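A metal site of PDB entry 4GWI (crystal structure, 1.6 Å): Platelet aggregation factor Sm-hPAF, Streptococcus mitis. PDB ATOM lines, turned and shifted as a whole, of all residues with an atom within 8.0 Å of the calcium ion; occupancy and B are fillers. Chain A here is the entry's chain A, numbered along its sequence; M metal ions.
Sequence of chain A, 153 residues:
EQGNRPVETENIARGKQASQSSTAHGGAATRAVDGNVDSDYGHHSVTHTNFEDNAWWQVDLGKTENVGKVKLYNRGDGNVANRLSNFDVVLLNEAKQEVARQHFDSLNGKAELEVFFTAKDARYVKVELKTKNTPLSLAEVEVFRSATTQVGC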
ATOM      1  N   ALA A  28     -15.019  26.088  -7.950  1.00  0.00           N
ATOM      2  CA  ALA A  28     -14.013  26.626  -7.068  1.00  0.00           C
ATOM      3  C   ALA A  28     -13.202  27.765  -7.682  1.00  0.00           C
ATOM      4  O   ALA A  28     -12.846  27.748  -8.876  1.00  0.00           O
ATOM      5  CB  ALA A  28     -13.013  25.479  -6.779  1.00  0.00           C
ATOM      6  N   ALA A  29     -12.946  28.780  -6.840  1.00  0.00           N
ATOM      7  CA  ALA A  29     -12.248  29.979  -7.311  1.00  0.00           C
ATOM      8  C   ALA A  29     -10.864  29.651  -7.883  1.00  0.00           C
ATOM      9  O   ALA A  29     -10.431  30.336  -8.812  1.00  0.00           O
ATOM     10  CB  ALA A  29     -12.016  30.949  -6.115  1.00  0.00           C
ATOM     11  N   THR A  30     -10.265  28.572  -7.394  1.00  0.00           N
ATOM     12  CA  THR A  30      -8.902  28.225  -7.884  1.00  0.00           C
ATOM     13  C   THR A  30      -8.964  27.712  -9.331  1.00  0.00           C
ATOM     14  O   THR A  30      -7.913  27.693  -9.990  1.00  0.00           O
ATOM     15  CB  THR A  30      -8.222  27.191  -7.013  1.00  0.00           C
ATOM     16  OG1 THR A  30      -9.143  26.111  -6.740  1.00  0.00           O
ATOM     17  CG2 THR A  30      -7.877  27.776  -5.705  1.00  0.00           C
ATOM     18  N   ARG A  31     -10.162  27.447  -9.867  1.00  0.00           N
ATOM     19  CA  ARG A  31     -10.196  27.045 -11.319  1.00  0.00           C
ATOM     20  C   ARG A  31      -9.785  28.126 -12.265  1.00  0.00           C
ATOM     21  O   ARG A  31      -9.455  27.888 -13.453  1.00  0.00           O
ATOM     22  CB  ARG A  31     -11.603  26.571 -11.652  1.00  0.00           C
ATOM     23  CG  ARG A  31     -11.921  25.251 -10.959  1.00  0.00           C
ATOM     24  CD  ARG A  31     -13.393  24.922 -11.242  1.00  0.00           C
ATOM     25  NE  ARG A  31     -13.666  23.605 -10.589  1.00  0.00           N
ATOM     26  CZ  ARG A  31     -14.801  22.932 -10.855  1.00  0.00           C
ATOM     27  NH1 ARG A  31     -14.978  21.673 -10.306  1.00  0.00           N
ATOM     28  NH2 ARG A  31     -15.768  23.445 -11.635  1.00  0.00           N
ATOM     29  N   ALA A  32      -9.787  29.425 -11.833  1.00  0.00           N
ATOM     30  CA  ALA A  32      -9.370  30.481 -12.760  1.00  0.00           C
ATOM     31  C   ALA A  32      -7.865  30.739 -12.713  1.00  0.00           C
ATOM     32  O   ALA A  32      -7.390  31.543 -13.496  1.00  0.00           O
ATOM     33  CB  ALA A  32     -10.157  31.843 -12.396  1.00  0.00           C
ATOM     34  N   VAL A  33      -7.176  30.002 -11.836  1.00  0.00           N
ATOM     35  CA  VAL A  33      -5.686  30.123 -11.835  1.00  0.00           C
ATOM     36  C   VAL A  33      -5.016  28.728 -11.899  1.00  0.00           C
ATOM     37  O   VAL A  33      -3.866  28.527 -11.475  1.00  0.00           O
ATOM     38  CB  VAL A  33      -5.154  30.951 -10.602  1.00  0.00           C
ATOM     39  CG1 VAL A  33      -5.606  32.425 -10.815  1.00  0.00           C
ATOM     40  CG2 VAL A  33      -5.627  30.322  -9.289  1.00  0.00           C
ATOM     41  N   ASP A  34      -5.717  27.813 -12.573  1.00  0.00           N
ATOM     42  CA  ASP A  34      -5.177  26.446 -12.626  1.00  0.00           C
ATOM     43  C   ASP A  34      -4.393  26.209 -13.899  1.00  0.00           C
ATOM     44  O   ASP A  34      -3.996  25.005 -14.109  1.00  0.00           O
ATOM     45  CB  ASP A  34      -6.332  25.413 -12.481  1.00  0.00           C
ATOM     46  CG  ASP A  34      -7.317  25.449 -13.645  1.00  0.00           C
ATOM     47  OD1 ASP A  34      -7.252  26.250 -14.554  1.00  0.00           O
ATOM     48  OD2 ASP A  34      -8.218  24.544 -13.616  1.00  0.00           O
ATOM     49  N   GLY A  35      -4.140  27.200 -14.749  1.00  0.00           N
ATOM     50  CA  GLY A  35      -3.314  27.007 -15.926  1.00  0.00           C
ATOM     51  C   GLY A  35      -4.050  26.345 -17.032  1.00  0.00           C
ATOM     52  O   GLY A  35      -3.399  25.845 -18.004  1.00  0.00           O
ATOM     53  N   ASN A  36      -5.384  26.422 -17.057  1.00  0.00           N
ATOM     54  CA  ASN A  36      -6.193  25.812 -18.115  1.00  0.00           C
ATOM     55  C   ASN A  36      -7.262  26.766 -18.531  1.00  0.00           C
ATOM     56  O   ASN A  36      -8.203  27.077 -17.695  1.00  0.00           O
ATOM     57  CB  ASN A  36      -6.811  24.532 -17.504  1.00  0.00           C
ATOM     58  CG  ASN A  36      -7.583  23.730 -18.564  1.00  0.00           C
ATOM     59  OD1 ASN A  36      -7.839  24.212 -19.665  1.00  0.00           O
ATOM     60  ND2 ASN A  36      -7.995  22.496 -18.144  1.00  0.00           N
ATOM     61  N   VAL A  37      -7.210  27.300 -19.743  1.00  0.00           N
ATOM     62  CA  VAL A  37      -8.199  28.269 -20.234  1.00  0.00           C
ATOM     63  C   VAL A  37      -9.483  27.652 -20.838  1.00  0.00           C
ATOM     64  O   VAL A  37     -10.325  28.372 -21.351  1.00  0.00           O
ATOM     65  CB  VAL A  37      -7.606  29.275 -21.227  1.00  0.00           C
ATOM     66  CG1 VAL A  37      -6.402  29.972 -20.582  1.00  0.00           C
ATOM     67  CG2 VAL A  37      -7.160  28.532 -22.576  1.00  0.00           C
ATOM     68  N   ASP A  38      -9.546  26.302 -20.817  1.00  0.00           N
ATOM     69  CA  ASP A  38     -10.770  25.633 -21.361  1.00  0.00           C
ATOM     70  C   ASP A  38     -12.034  26.222 -20.802  1.00  0.00           C
ATOM     71  O   ASP A  38     -12.203  26.230 -19.573  1.00  0.00           O
ATOM     72  CB  ASP A  38     -10.676  24.110 -21.043  1.00  0.00           C
ATOM     73  CG  ASP A  38     -11.705  23.307 -21.780  1.00  0.00           C
ATOM     74  OD1 ASP A  38     -11.395  22.087 -22.038  1.00  0.00           O
ATOM     75  OD2 ASP A  38     -12.812  23.768 -22.071  1.00  0.00           O
ATOM     76  N   SER A  39     -12.876  26.761 -21.691  1.00  0.00           N
ATOM     77  CA  SER A  39     -14.014  27.518 -21.254  1.00  0.00           C
ATOM     78  C   SER A  39     -15.325  26.773 -21.074  1.00  0.00           C
ATOM     79  O   SER A  39     -16.370  27.352 -20.766  1.00  0.00           O
ATOM     80  CB  SER A  39     -14.181  28.702 -22.200  1.00  0.00           C
ATOM     81  OG  SER A  39     -14.616  28.190 -23.473  1.00  0.00           O
ATOM     82  N   HIS A  43     -15.815  20.768 -18.339  1.00  0.00           N
ATOM     83  CA  HIS A  43     -14.443  20.323 -18.250  1.00  0.00           C
ATOM     84  C   HIS A  43     -13.691  20.767 -16.961  1.00  0.00           C
ATOM     85  O   HIS A  43     -12.502  20.498 -16.759  1.00  0.00           O
ATOM     86  CB  HIS A  43     -13.677  20.782 -19.485  1.00  0.00           C
ATOM     87  CG  HIS A  43     -14.262  20.266 -20.772  1.00  0.00           C
ATOM     88  ND1 HIS A  43     -13.778  20.704 -21.944  1.00  0.00           N
ATOM     89  CD2 HIS A  43     -15.234  19.326 -21.034  1.00  0.00           C
ATOM     90  CE1 HIS A  43     -14.505  20.125 -22.993  1.00  0.00           C
ATOM     91  NE2 HIS A  43     -15.364  19.256 -22.424  1.00  0.00           N
ATOM     92  N   HIS A  44     -14.507  21.414 -16.049  1.00  0.00           N
ATOM     93  CA  HIS A  44     -14.078  21.620 -14.642  1.00  0.00           C
ATOM     94  C   HIS A  44     -13.032  22.697 -14.423  1.00  0.00           C
ATOM     95  O   HIS A  44     -12.386  22.654 -13.379  1.00  0.00           O
ATOM     96  CB  HIS A  44     -13.597  20.305 -13.965  1.00  0.00           C
ATOM     97  CG  HIS A  44     -14.586  19.177 -14.088  1.00  0.00           C
ATOM     98  ND1 HIS A  44     -15.836  19.296 -13.671  1.00  0.00           N
ATOM     99  CD2 HIS A  44     -14.420  17.864 -14.552  1.00  0.00           C
ATOM    100  CE1 HIS A  44     -16.492  18.101 -13.835  1.00  0.00           C
ATOM    101  NE2 HIS A  44     -15.632  17.232 -14.378  1.00  0.00           N
ATOM    102  N   SER A  45     -12.823  23.583 -15.387  1.00  0.00           N
ATOM    103  CA  SER A  45     -11.748  24.587 -15.201  1.00  0.00           C
ATOM    104  C   SER A  45     -12.369  26.001 -15.201  1.00  0.00           C
ATOM    105  O   SER A  45     -11.632  26.982 -15.435  1.00  0.00           O
ATOM    106  CB  SER A  45     -10.656  24.428 -16.299  1.00  0.00           C
ATOM    107  OG  SER A  45      -9.463  25.139 -15.817  1.00  0.00           O
ATOM    108  N   VAL A  46     -13.679  26.106 -14.889  1.00  0.00           N
ATOM    109  CA  VAL A  46     -14.348  27.418 -14.881  1.00  0.00           C
ATOM    110  C   VAL A  46     -14.976  27.597 -13.500  1.00  0.00           C
ATOM    111  O   VAL A  46     -15.558  26.662 -12.919  1.00  0.00           O
ATOM    112  CB  VAL A  46     -15.471  27.479 -15.976  1.00  0.00           C
ATOM    113  CG1 VAL A  46     -16.222  28.818 -15.938  1.00  0.00           C
ATOM    114  CG2 VAL A  46     -14.895  27.170 -17.415  1.00  0.00           C
ATOM    115  N   THR A  47     -14.850  28.842 -12.987  1.00  0.00           N
ATOM    116  CA  THR A  47     -15.383  29.084 -11.610  1.00  0.00           C
ATOM    117  C   THR A  47     -16.895  29.388 -11.706  1.00  0.00           C
ATOM    118  O   THR A  47     -17.454  29.556 -12.810  1.00  0.00           O
ATOM    119  CB  THR A  47     -14.757  30.363 -11.031  1.00  0.00           C
ATOM    120  OG1 THR A  47     -15.148  31.538 -11.787  1.00  0.00           O
ATOM    121  CG2 THR A  47     -13.198  30.373 -11.081  1.00  0.00           C
ATOM    122  N   TYR A  73     -10.489  35.190 -19.335  1.00  0.00           N
ATOM    123  CA  TYR A  73     -11.059  34.219 -20.319  1.00  0.00           C
ATOM    124  C   TYR A  73     -12.409  33.847 -19.834  1.00  0.00           C
ATOM    125  O   TYR A  73     -12.571  33.377 -18.682  1.00  0.00           O
ATOM    126  CB  TYR A  73     -10.178  32.965 -20.376  1.00  0.00           C
ATOM    127  CG  TYR A  73      -8.774  33.189 -20.890  1.00  0.00           C
ATOM    128  CD1 TYR A  73      -8.464  32.767 -22.180  1.00  0.00           C
ATOM    129  CD2 TYR A  73      -7.780  33.830 -20.110  1.00  0.00           C
ATOM    130  CE1 TYR A  73      -7.179  32.945 -22.647  1.00  0.00           C
ATOM    131  CE2 TYR A  73      -6.491  34.025 -20.601  1.00  0.00           C
ATOM    132  CZ  TYR A  73      -6.225  33.573 -21.882  1.00  0.00           C
ATOM    133  OH  TYR A  73      -4.944  33.685 -22.357  1.00  0.00           O
ATOM    134  N   LEU A 138     -15.415  32.534 -14.451  1.00  0.00           N
ATOM    135  CA  LEU A 138     -14.243  32.850 -15.269  1.00  0.00           C
ATOM    136  C   LEU A 138     -13.517  31.536 -15.597  1.00  0.00           C
ATOM    137  O   LEU A 138     -13.315  30.675 -14.685  1.00  0.00           O
ATOM    138  CB  LEU A 138     -13.271  33.723 -14.421  1.00  0.00           C
ATOM    139  CG  LEU A 138     -13.910  35.065 -14.133  1.00  0.00           C
ATOM    140  CD1 LEU A 138     -13.193  35.678 -12.882  1.00  0.00           C
ATOM    141  CD2 LEU A 138     -13.672  35.989 -15.334  1.00  0.00           C
ATOM    142  N   ALA A 139     -13.150  31.360 -16.895  1.00  0.00           N
ATOM    143  CA  ALA A 139     -12.366  30.158 -17.139  1.00  0.00           C
ATOM    144  C   ALA A 139     -10.914  30.287 -16.701  1.00  0.00           C
ATOM    145  O   ALA A 139     -10.257  29.369 -16.363  1.00  0.00           O
ATOM    146  CB  ALA A 139     -12.386  29.954 -18.687  1.00  0.00           C
ATOM    147  N   GLU A 140     -10.392  31.543 -16.737  1.00  0.00           N
ATOM    148  CA  GLU A 140      -8.985  31.756 -16.300  1.00  0.00           C
ATOM    149  C   GLU A 140      -8.794  33.285 -16.192  1.00  0.00           C
ATOM    150  O   GLU A 140      -9.415  34.042 -16.937  1.00  0.00           O
ATOM    151  CB  GLU A 140      -8.009  31.207 -17.411  1.00  0.00           C
ATOM    152  CG  GLU A 140      -6.583  31.035 -16.828  1.00  0.00           C
ATOM    153  CD  GLU A 140      -6.354  29.800 -15.932  1.00  0.00           C
ATOM    154  OE1 GLU A 140      -7.263  29.033 -15.569  1.00  0.00           O
ATOM    155  OE2 GLU A 140      -5.195  29.656 -15.468  1.00  0.00           O
ATOM    156  N   VAL A 141      -7.933  33.637 -15.214  1.00  0.00           N
ATOM    157  CA  VAL A 141      -7.428  35.043 -15.188  1.00  0.00           C
ATOM    158  C   VAL A 141      -5.899  34.916 -15.141  1.00  0.00           C
ATOM    159  O   VAL A 141      -5.329  34.187 -14.277  1.00  0.00           O
ATOM    160  CB  VAL A 141      -7.918  35.683 -13.866  1.00  0.00           C
ATOM    161  CG1 VAL A 141      -7.281  37.094 -13.755  1.00  0.00           C
ATOM    162  CG2 VAL A 141      -9.447  35.859 -13.880  1.00  0.00           C
HETATM  163 CA    CA M   1      -9.127  27.458 -15.631  1.00  0.00          CA
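The backbone carbonyl oxygen (O) of Val 46 lies close to the guanidinium group (NH2) of Arg 31, at 3.5 Å.
The guanidinium group of Arg 31 is in hydrogen-bond range of the backbone carbonyl oxygen of His 44, at 3.2 Å.
The backbone NH (N) of Asp 38 sits at hydrogen-bond distance from the side-chain amide oxygen (OD1) of Asn 36 (2.9 Å).
The backbone carbonyl oxygen (O) of Tyr 73 sits at hydrogen-bond distance from the backbone NH (N) of Ala 139.
OE2 of Glu 140 sits at hydrogen-bond distance from N of Gly 35 (2.8 Å).
O of Glu 140 lies within hydrogen-bond range of N of Tyr 73 (2.9 Å).
The nearest printed residue that does not touch the calcium ion is Ala 32 (4.2 Å).
The calcium ion is bound by the backbone carbonyl oxygen (O) of Arg 31 (2.2 Å), the backbone carbonyl oxygen (O) of Asn 36 (2.3 Å), the backbone carbonyl oxygen (O) of Ala 139 (2.3 Å), the side-chain hydroxyl (OG) of Ser 45 (2.4 Å), the side-chain carboxylate (OE1) of Glu 140 (2.4 Å), the side-chain carboxylate (OD1) of Asp 34 (2.5 Å) and the backbone carbonyl oxygen (O) of Ser 45 (2.6 Å).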
